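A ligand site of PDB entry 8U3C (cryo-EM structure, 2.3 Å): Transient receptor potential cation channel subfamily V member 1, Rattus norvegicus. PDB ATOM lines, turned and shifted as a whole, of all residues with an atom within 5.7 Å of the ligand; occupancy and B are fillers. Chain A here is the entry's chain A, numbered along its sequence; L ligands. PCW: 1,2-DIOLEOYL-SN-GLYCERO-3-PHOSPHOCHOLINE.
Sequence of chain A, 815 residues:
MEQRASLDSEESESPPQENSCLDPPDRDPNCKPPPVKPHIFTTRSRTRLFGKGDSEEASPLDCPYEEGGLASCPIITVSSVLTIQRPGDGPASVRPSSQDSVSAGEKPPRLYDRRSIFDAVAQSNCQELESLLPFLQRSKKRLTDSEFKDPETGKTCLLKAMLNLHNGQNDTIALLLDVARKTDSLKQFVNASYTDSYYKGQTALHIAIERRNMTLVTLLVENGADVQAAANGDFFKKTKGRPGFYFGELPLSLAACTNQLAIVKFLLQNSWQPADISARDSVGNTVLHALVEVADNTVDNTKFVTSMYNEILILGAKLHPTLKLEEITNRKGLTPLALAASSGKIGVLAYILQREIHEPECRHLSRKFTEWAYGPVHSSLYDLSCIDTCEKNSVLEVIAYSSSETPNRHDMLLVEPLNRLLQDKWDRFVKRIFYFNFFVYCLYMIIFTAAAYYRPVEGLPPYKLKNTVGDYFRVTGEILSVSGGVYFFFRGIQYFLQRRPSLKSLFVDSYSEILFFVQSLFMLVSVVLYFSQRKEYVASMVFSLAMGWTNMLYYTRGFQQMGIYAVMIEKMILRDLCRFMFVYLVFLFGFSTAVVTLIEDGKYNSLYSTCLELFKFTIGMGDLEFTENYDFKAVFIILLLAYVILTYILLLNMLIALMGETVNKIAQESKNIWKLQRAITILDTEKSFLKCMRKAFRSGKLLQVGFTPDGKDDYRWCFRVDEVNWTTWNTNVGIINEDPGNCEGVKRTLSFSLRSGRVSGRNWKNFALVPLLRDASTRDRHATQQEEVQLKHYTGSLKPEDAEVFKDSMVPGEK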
ATOM      1  N   PHE A 436      -4.915  31.233 -17.720  1.00  0.00           N
ATOM      2  CA  PHE A 436      -4.996  30.158 -16.745  1.00  0.00           C
ATOM      3  C   PHE A 436      -4.940  28.791 -17.428  1.00  0.00           C
ATOM      4  O   PHE A 436      -4.278  27.863 -16.928  1.00  0.00           O
ATOM      5  CB  PHE A 436      -6.276  30.280 -15.921  1.00  0.00           C
ATOM      6  CG  PHE A 436      -6.429  29.209 -14.873  1.00  0.00           C
ATOM      7  CD1 PHE A 436      -5.723  29.284 -13.687  1.00  0.00           C
ATOM      8  CD2 PHE A 436      -7.257  28.134 -15.088  1.00  0.00           C
ATOM      9  CE1 PHE A 436      -5.850  28.300 -12.731  1.00  0.00           C
ATOM     10  CE2 PHE A 436      -7.401  27.148 -14.134  1.00  0.00           C
ATOM     11  CZ  PHE A 436      -6.695  27.232 -12.959  1.00  0.00           C
ATOM     12  N   ASN A 437      -5.636  28.643 -18.553  1.00  0.00           N
ATOM     13  CA  ASN A 437      -5.572  27.385 -19.285  1.00  0.00           C
ATOM     14  C   ASN A 437      -4.152  27.073 -19.748  1.00  0.00           C
ATOM     15  O   ASN A 437      -3.690  25.934 -19.660  1.00  0.00           O
ATOM     16  CB  ASN A 437      -6.520  27.424 -20.480  1.00  0.00           C
ATOM     17  CG  ASN A 437      -7.971  27.404 -20.068  1.00  0.00           C
ATOM     18  OD1 ASN A 437      -8.312  27.028 -18.943  1.00  0.00           O
ATOM     19  ND2 ASN A 437      -8.857  27.809 -20.977  1.00  0.00           N
ATOM     20  N   PHE A 438      -3.453  28.096 -20.250  1.00  0.00           N
ATOM     21  CA  PHE A 438      -2.069  27.906 -20.688  1.00  0.00           C
ATOM     22  C   PHE A 438      -1.181  27.492 -19.523  1.00  0.00           C
ATOM     23  O   PHE A 438      -0.335  26.598 -19.677  1.00  0.00           O
ATOM     24  CB  PHE A 438      -1.564  29.203 -21.324  1.00  0.00           C
ATOM     25  CG  PHE A 438      -0.222  29.074 -22.014  1.00  0.00           C
ATOM     26  CD1 PHE A 438       0.376  27.839 -22.206  1.00  0.00           C
ATOM     27  CD2 PHE A 438       0.428  30.207 -22.466  1.00  0.00           C
ATOM     28  CE1 PHE A 438       1.599  27.748 -22.844  1.00  0.00           C
ATOM     29  CE2 PHE A 438       1.649  30.122 -23.090  1.00  0.00           C
ATOM     30  CZ  PHE A 438       2.241  28.885 -23.276  1.00  0.00           C
ATOM     31  N   VAL A 440      -2.081  25.905 -16.808  1.00  0.00           N
ATOM     32  CA  VAL A 440      -2.465  24.535 -16.380  1.00  0.00           C
ATOM     33  C   VAL A 440      -1.859  23.555 -17.383  1.00  0.00           C
ATOM     34  O   VAL A 440      -1.414  22.514 -16.938  1.00  0.00           O
ATOM     35  CB  VAL A 440      -3.987  24.343 -16.271  1.00  0.00           C
ATOM     36  CG1 VAL A 440      -4.358  22.869 -16.152  1.00  0.00           C
ATOM     37  CG2 VAL A 440      -4.565  25.122 -15.101  1.00  0.00           C
ATOM     38  N   TYR A 441      -1.873  23.865 -18.685  1.00  0.00           N
ATOM     39  CA  TYR A 441      -1.287  22.960 -19.674  1.00  0.00           C
ATOM     40  C   TYR A 441       0.229  22.875 -19.515  1.00  0.00           C
ATOM     41  O   TYR A 441       0.818  21.800 -19.680  1.00  0.00           O
ATOM     42  CB  TYR A 441      -1.645  23.417 -21.081  1.00  0.00           C
ATOM     43  CG  TYR A 441      -1.191  22.437 -22.135  1.00  0.00           C
ATOM     44  CD1 TYR A 441      -1.810  21.199 -22.273  1.00  0.00           C
ATOM     45  CD2 TYR A 441      -0.135  22.742 -22.989  1.00  0.00           C
ATOM     46  CE1 TYR A 441      -1.396  20.302 -23.236  1.00  0.00           C
ATOM     47  CE2 TYR A 441       0.285  21.839 -23.948  1.00  0.00           C
ATOM     48  CZ  TYR A 441      -0.349  20.625 -24.066  1.00  0.00           C
ATOM     49  OH  TYR A 441       0.070  19.735 -25.023  1.00  0.00           O
ATOM     50  N   LEU A 443       1.911  23.233 -16.713  1.00  0.00           N
ATOM     51  CA  LEU A 443       2.137  22.368 -15.555  1.00  0.00           C
ATOM     52  C   LEU A 443       1.939  20.908 -15.916  1.00  0.00           C
ATOM     53  O   LEU A 443       2.722  20.041 -15.499  1.00  0.00           O
ATOM     54  CB  LEU A 443       1.209  22.766 -14.416  1.00  0.00           C
ATOM     55  CG  LEU A 443       1.580  24.012 -13.603  1.00  0.00           C
ATOM     56  CD1 LEU A 443       0.521  24.258 -12.544  1.00  0.00           C
ATOM     57  CD2 LEU A 443       2.958  23.866 -12.973  1.00  0.00           C
ATOM     58  N   TYR A 444       0.890  20.608 -16.671  1.00  0.00           N
ATOM     59  CA  TYR A 444       0.625  19.227 -17.071  1.00  0.00           C
ATOM     60  C   TYR A 444       1.783  18.668 -17.887  1.00  0.00           C
ATOM     61  O   TYR A 444       2.217  17.536 -17.660  1.00  0.00           O
ATOM     62  CB  TYR A 444      -0.677  19.167 -17.871  1.00  0.00           C
ATOM     63  CG  TYR A 444      -0.855  17.895 -18.669  1.00  0.00           C
ATOM     64  CD1 TYR A 444      -1.092  16.682 -18.037  1.00  0.00           C
ATOM     65  CD2 TYR A 444      -0.773  17.910 -20.049  1.00  0.00           C
ATOM     66  CE1 TYR A 444      -1.254  15.531 -18.765  1.00  0.00           C
ATOM     67  CE2 TYR A 444      -0.941  16.766 -20.781  1.00  0.00           C
ATOM     68  CZ  TYR A 444      -1.181  15.572 -20.134  1.00  0.00           C
ATOM     69  OH  TYR A 444      -1.335  14.422 -20.870  1.00  0.00           O
ATOM     70  N   ILE A 447       4.864  18.037 -15.653  1.00  0.00           N
ATOM     71  CA  ILE A 447       4.716  16.841 -14.831  1.00  0.00           C
ATOM     72  C   ILE A 447       4.821  15.583 -15.688  1.00  0.00           C
ATOM     73  O   ILE A 447       5.440  14.600 -15.279  1.00  0.00           O
ATOM     74  CB  ILE A 447       3.388  16.887 -14.053  1.00  0.00           C
ATOM     75  CG1 ILE A 447       3.487  17.892 -12.901  1.00  0.00           C
ATOM     76  CG2 ILE A 447       3.022  15.517 -13.515  1.00  0.00           C
ATOM     77  CD1 ILE A 447       2.148  18.404 -12.429  1.00  0.00           C
ATOM     78  N   LEU A 480      -1.360  11.787 -12.741  1.00  0.00           N
ATOM     79  CA  LEU A 480      -1.793  13.070 -13.310  1.00  0.00           C
ATOM     80  C   LEU A 480      -1.694  13.056 -14.829  1.00  0.00           C
ATOM     81  O   LEU A 480      -2.574  13.595 -15.513  1.00  0.00           O
ATOM     82  CB  LEU A 480      -0.959  14.213 -12.722  1.00  0.00           C
ATOM     83  CG  LEU A 480      -1.092  14.456 -11.220  1.00  0.00           C
ATOM     84  CD1 LEU A 480      -0.188  15.584 -10.778  1.00  0.00           C
ATOM     85  CD2 LEU A 480      -2.536  14.758 -10.849  1.00  0.00           C
ATOM     86  N   SER A 483      -4.586  11.082 -16.149  1.00  0.00           N
ATOM     87  CA  SER A 483      -5.810  11.855 -15.962  1.00  0.00           C
ATOM     88  C   SER A 483      -5.936  12.937 -17.023  1.00  0.00           C
ATOM     89  O   SER A 483      -7.025  13.156 -17.573  1.00  0.00           O
ATOM     90  CB  SER A 483      -5.839  12.468 -14.568  1.00  0.00           C
ATOM     91  OG  SER A 483      -4.882  13.505 -14.450  1.00  0.00           O
ATOM     92  N   GLY A 484      -4.843  13.639 -17.321  1.00  0.00           N
ATOM     93  CA  GLY A 484      -4.880  14.629 -18.379  1.00  0.00           C
ATOM     94  C   GLY A 484      -5.174  14.024 -19.745  1.00  0.00           C
ATOM     95  O   GLY A 484      -5.905  14.602 -20.546  1.00  0.00           O
ATOM     96  N   TYR A 487      -8.806  13.322 -19.843  1.00  0.00           N
ATOM     97  CA  TYR A 487      -9.497  14.632 -19.930  1.00  0.00           C
ATOM     98  C   TYR A 487      -9.504  15.114 -21.374  1.00  0.00           C
ATOM     99  O   TYR A 487     -10.527  15.636 -21.796  1.00  0.00           O
ATOM    100  CB  TYR A 487      -8.804  15.706 -19.105  1.00  0.00           C
ATOM    101  CG  TYR A 487      -9.221  17.112 -19.429  1.00  0.00           C
ATOM    102  CD1 TYR A 487     -10.491  17.570 -19.125  1.00  0.00           C
ATOM    103  CD2 TYR A 487      -8.373  17.961 -20.110  1.00  0.00           C
ATOM    104  CE1 TYR A 487     -10.882  18.863 -19.439  1.00  0.00           C
ATOM    105  CE2 TYR A 487      -8.751  19.257 -20.439  1.00  0.00           C
ATOM    106  CZ  TYR A 487     -10.006  19.703 -20.098  1.00  0.00           C
ATOM    107  OH  TYR A 487     -10.401  20.975 -20.420  1.00  0.00           O
ATOM    108  N   PHE A 488      -8.379  15.008 -22.073  1.00  0.00           N
ATOM    109  CA  PHE A 488      -8.297  15.469 -23.458  1.00  0.00           C
ATOM    110  C   PHE A 488      -9.053  14.535 -24.400  1.00  0.00           C
ATOM    111  O   PHE A 488      -9.667  14.984 -25.372  1.00  0.00           O
ATOM    112  CB  PHE A 488      -6.835  15.601 -23.889  1.00  0.00           C
ATOM    113  CG  PHE A 488      -6.173  16.857 -23.401  1.00  0.00           C
ATOM    114  CD1 PHE A 488      -6.700  18.093 -23.711  1.00  0.00           C
ATOM    115  CD2 PHE A 488      -5.027  16.798 -22.630  1.00  0.00           C
ATOM    116  CE1 PHE A 488      -6.096  19.250 -23.268  1.00  0.00           C
ATOM    117  CE2 PHE A 488      -4.423  17.955 -22.187  1.00  0.00           C
ATOM    118  CZ  PHE A 488      -4.966  19.176 -22.501  1.00  0.00           C
ATOM    119  N   ARG A 491     -12.636  15.459 -24.001  1.00  0.00           N
ATOM    120  CA  ARG A 491     -12.837  16.823 -24.577  1.00  0.00           C
ATOM    121  C   ARG A 491     -12.882  16.717 -26.095  1.00  0.00           C
ATOM    122  O   ARG A 491     -13.610  17.509 -26.697  1.00  0.00           O
ATOM    123  CB  ARG A 491     -11.719  17.773 -24.150  1.00  0.00           C
ATOM    124  CG  ARG A 491     -11.905  18.410 -22.779  1.00  0.00           C
ATOM    125  CD  ARG A 491     -13.051  19.405 -22.729  1.00  0.00           C
ATOM    126  NE  ARG A 491     -13.008  20.378 -23.815  1.00  0.00           N
ATOM    127  CZ  ARG A 491     -12.031  21.250 -24.028  1.00  0.00           C
ATOM    128  NH1 ARG A 491     -11.220  21.602 -23.051  1.00  0.00           N
ATOM    129  NH2 ARG A 491     -11.876  21.783 -25.226  1.00  0.00           N
ATOM    130  N   SER A 512      -6.154  21.603 -34.498  1.00  0.00           N
ATOM    131  CA  SER A 512      -5.824  21.590 -33.054  1.00  0.00           C
ATOM    132  C   SER A 512      -6.589  20.473 -32.348  1.00  0.00           C
ATOM    133  O   SER A 512      -5.954  19.725 -31.616  1.00  0.00           O
ATOM    134  CB  SER A 512      -6.101  22.934 -32.407  1.00  0.00           C
ATOM    135  OG  SER A 512      -7.459  23.324 -32.587  1.00  0.00           O
ATOM    136  N   GLU A 513      -7.902  20.350 -32.566  1.00  0.00           N
ATOM    137  CA  GLU A 513      -8.720  19.354 -31.892  1.00  0.00           C
ATOM    138  C   GLU A 513      -8.239  17.940 -32.215  1.00  0.00           C
ATOM    139  O   GLU A 513      -8.091  17.100 -31.323  1.00  0.00           O
ATOM    140  CB  GLU A 513     -10.187  19.523 -32.299  1.00  0.00           C
ATOM    141  CG  GLU A 513     -10.883  20.711 -31.650  1.00  0.00           C
ATOM    142  CD  GLU A 513     -11.129  20.508 -30.173  1.00  0.00           C
ATOM    143  OE1 GLU A 513     -10.937  19.372 -29.688  1.00  0.00           O
ATOM    144  OE2 GLU A 513     -11.518  21.478 -29.496  1.00  0.00           O
ATOM    145  N   PHE A 516      -4.752  17.302 -30.396  1.00  0.00           N
ATOM    146  CA  PHE A 516      -4.903  17.009 -28.979  1.00  0.00           C
ATOM    147  C   PHE A 516      -5.566  15.644 -28.767  1.00  0.00           C
ATOM    148  O   PHE A 516      -5.175  14.884 -27.873  1.00  0.00           O
ATOM    149  CB  PHE A 516      -5.711  18.103 -28.301  1.00  0.00           C
ATOM    150  CG  PHE A 516      -4.900  19.309 -27.909  1.00  0.00           C
ATOM    151  CD1 PHE A 516      -4.559  20.274 -28.844  1.00  0.00           C
ATOM    152  CD2 PHE A 516      -4.471  19.476 -26.607  1.00  0.00           C
ATOM    153  CE1 PHE A 516      -3.812  21.379 -28.491  1.00  0.00           C
ATOM    154  CE2 PHE A 516      -3.713  20.581 -26.244  1.00  0.00           C
ATOM    155  CZ  PHE A 516      -3.392  21.524 -27.188  1.00  0.00           C
ATOM    156  N   TYR A 554      -0.323  25.697 -29.802  1.00  0.00           N
ATOM    157  CA  TYR A 554      -1.716  26.114 -29.843  1.00  0.00           C
ATOM    158  C   TYR A 554      -1.931  27.411 -29.086  1.00  0.00           C
ATOM    159  O   TYR A 554      -2.708  28.272 -29.499  1.00  0.00           O
ATOM    160  CB  TYR A 554      -2.612  25.020 -29.288  1.00  0.00           C
ATOM    161  CG  TYR A 554      -4.009  25.498 -28.956  1.00  0.00           C
ATOM    162  CD1 TYR A 554      -5.007  25.499 -29.921  1.00  0.00           C
ATOM    163  CD2 TYR A 554      -4.321  25.950 -27.683  1.00  0.00           C
ATOM    164  CE1 TYR A 554      -6.275  25.942 -29.619  1.00  0.00           C
ATOM    165  CE2 TYR A 554      -5.589  26.394 -27.381  1.00  0.00           C
ATOM    166  CZ  TYR A 554      -6.564  26.398 -28.352  1.00  0.00           C
ATOM    167  OH  TYR A 554      -7.826  26.834 -28.046  1.00  0.00           O
ATOM    168  N   TYR A 555      -1.237  27.573 -27.959  1.00  0.00           N
ATOM    169  CA  TYR A 555      -1.445  28.719 -27.096  1.00  0.00           C
ATOM    170  C   TYR A 555      -0.748  29.970 -27.588  1.00  0.00           C
ATOM    171  O   TYR A 555      -0.822  31.007 -26.916  1.00  0.00           O
ATOM    172  CB  TYR A 555      -0.998  28.384 -25.679  1.00  0.00           C
ATOM    173  CG  TYR A 555      -1.862  27.337 -25.030  1.00  0.00           C
ATOM    174  CD1 TYR A 555      -3.076  27.665 -24.438  1.00  0.00           C
ATOM    175  CD2 TYR A 555      -1.487  26.001 -25.022  1.00  0.00           C
ATOM    176  CE1 TYR A 555      -3.876  26.707 -23.860  1.00  0.00           C
ATOM    177  CE2 TYR A 555      -2.280  25.036 -24.442  1.00  0.00           C
ATOM    178  CZ  TYR A 555      -3.477  25.397 -23.868  1.00  0.00           C
ATOM    179  OH  TYR A 555      -4.266  24.439 -23.281  1.00  0.00           O
ATOM    180  N   ASP A 684     -15.712  29.519 -27.361  1.00  0.00           N
ATOM    181  CA  ASP A 684     -15.618  28.307 -26.561  1.00  0.00           C
ATOM    182  C   ASP A 684     -15.558  28.634 -25.073  1.00  0.00           C
ATOM    183  O   ASP A 684     -16.216  27.986 -24.260  1.00  0.00           O
ATOM    184  CB  ASP A 684     -14.379  27.502 -26.971  1.00  0.00           C
ATOM    185  CG  ASP A 684     -14.581  26.754 -28.276  1.00  0.00           C
ATOM    186  OD1 ASP A 684     -15.731  26.723 -28.775  1.00  0.00           O
ATOM    187  OD2 ASP A 684     -13.595  26.200 -28.795  1.00  0.00           O
HETATM  188  C1  PCW L   1      -5.736  23.248 -21.106  1.00  0.00           C
HETATM  189  C2  PCW L   1      -5.707  22.686 -19.688  1.00  0.00           C
HETATM  190  C3  PCW L   1      -6.557  23.587 -18.795  1.00  0.00           C
HETATM  191  C4  PCW L   1      -6.517  23.212 -25.716  1.00  0.00           C
HETATM  192  C5  PCW L   1      -7.215  22.032 -26.408  1.00  0.00           C
HETATM  193  C6  PCW L   1      -6.953  22.909 -28.658  1.00  0.00           C
HETATM  194  C7  PCW L   1      -8.364  21.115 -28.214  1.00  0.00           C
HETATM  195  C8  PCW L   1      -8.973  23.257 -27.459  1.00  0.00           C
HETATM  196  C11 PCW L   1      -8.742  23.357 -18.074  1.00  0.00           C
HETATM  197  C12 PCW L   1      -9.001  21.954 -17.531  1.00  0.00           C
HETATM  198  C13 PCW L   1      -8.557  21.891 -16.068  1.00  0.00           C
HETATM  199  C14 PCW L   1      -8.726  20.454 -15.576  1.00  0.00           C
HETATM  200  C31 PCW L   1      -5.455  20.417 -19.020  1.00  0.00           C
HETATM  201  C32 PCW L   1      -6.068  19.740 -17.784  1.00  0.00           C
HETATM  202  C33 PCW L   1      -5.510  18.335 -17.579  1.00  0.00           C
HETATM  203  C34 PCW L   1      -4.165  18.413 -16.872  1.00  0.00           C
HETATM  204  C35 PCW L   1      -4.253  17.719 -15.519  1.00  0.00           C
HETATM  205  C36 PCW L   1      -2.872  17.737 -14.876  1.00  0.00           C
HETATM  206  C37 PCW L   1      -2.729  18.939 -13.963  1.00  0.00           C
HETATM  207  C38 PCW L   1      -1.286  19.437 -14.057  1.00  0.00           C
HETATM  208  N   PCW L   1      -7.859  22.354 -27.663  1.00  0.00           N
HETATM  209  O2  PCW L   1      -6.216  21.385 -19.718  1.00  0.00           O
HETATM  210  O3  PCW L   1      -7.891  23.514 -19.181  1.00  0.00           O
HETATM  211  O11 PCW L   1      -9.227  24.299 -17.568  1.00  0.00           O
HETATM  212  O31 PCW L   1      -4.371  20.125 -19.407  1.00  0.00           O
HETATM  213  O1P PCW L   1      -7.075  25.140 -23.255  1.00  0.00           O
HETATM  214  O2P PCW L   1      -8.733  23.671 -23.530  1.00  0.00           O
HETATM  215  O3P PCW L   1      -7.003  23.069 -21.701  1.00  0.00           O
HETATM  216  O4P PCW L   1      -6.404  22.903 -24.355  1.00  0.00           O
HETATM  217  P   PCW L   1      -7.308  23.704 -23.208  1.00  0.00           P
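The guanidinium group of Arg 491 lies within salt-bridge range of an oxygen (O2P) of the ligand, 3.3 Å away. An oxygen (O4P) of the ligand is in hydrogen-bond range of the side-chain hydroxyl (OH) of Tyr 555, 2.8 Å away. OD1 of Asn 437 lies close to O11 of the ligand (3.2 Å).
The side-chain hydroxyl of Tyr 487 is in hydrogen-bond range of the guanidinium group of Arg 491 (2.8 Å).
Val 440 touches the ligand. CD1 of Tyr 441 touches O31 of the ligand, 3.99 Å away. Tyr 444 touches the ligand (CA to C38, 3.6 Å). Ile 447 touches the ligand. Gly 484 touches the ligand (CA to C33, 3.8 Å). Tyr 487 touches the ligand (OH to C12, 3.4 Å). CZ of Phe 488 touches O31 of the ligand (3.3 Å). CB of Ser 512 touches C6 of the ligand (3.8 Å). OE2 of Glu 513 touches C7 of the ligand, 3.4 Å away. CE1 of Phe 516 touches C6 of the ligand, 3.5 Å away. CE1 of Tyr 554 touches C6 of the ligand, at 3.3 Å. Hydrophobic or aromatic side chains that line the ligand: Val 440, Tyr 441, Tyr 444, Ile 447, Tyr 487, Phe 488, Phe 516, Tyr 554 and Tyr 555. Within 4 Å of the ligand: Asn 437, Val 440, Tyr 441, Tyr 444, Ile 447, Gly 484, Tyr 487, Phe 488, Arg 491, Ser 512, Glu 513, Phe 516, Tyr 554 and Tyr 555. The nearest printed residue that does not touch the ligand is Leu 443 (4.003 Å).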
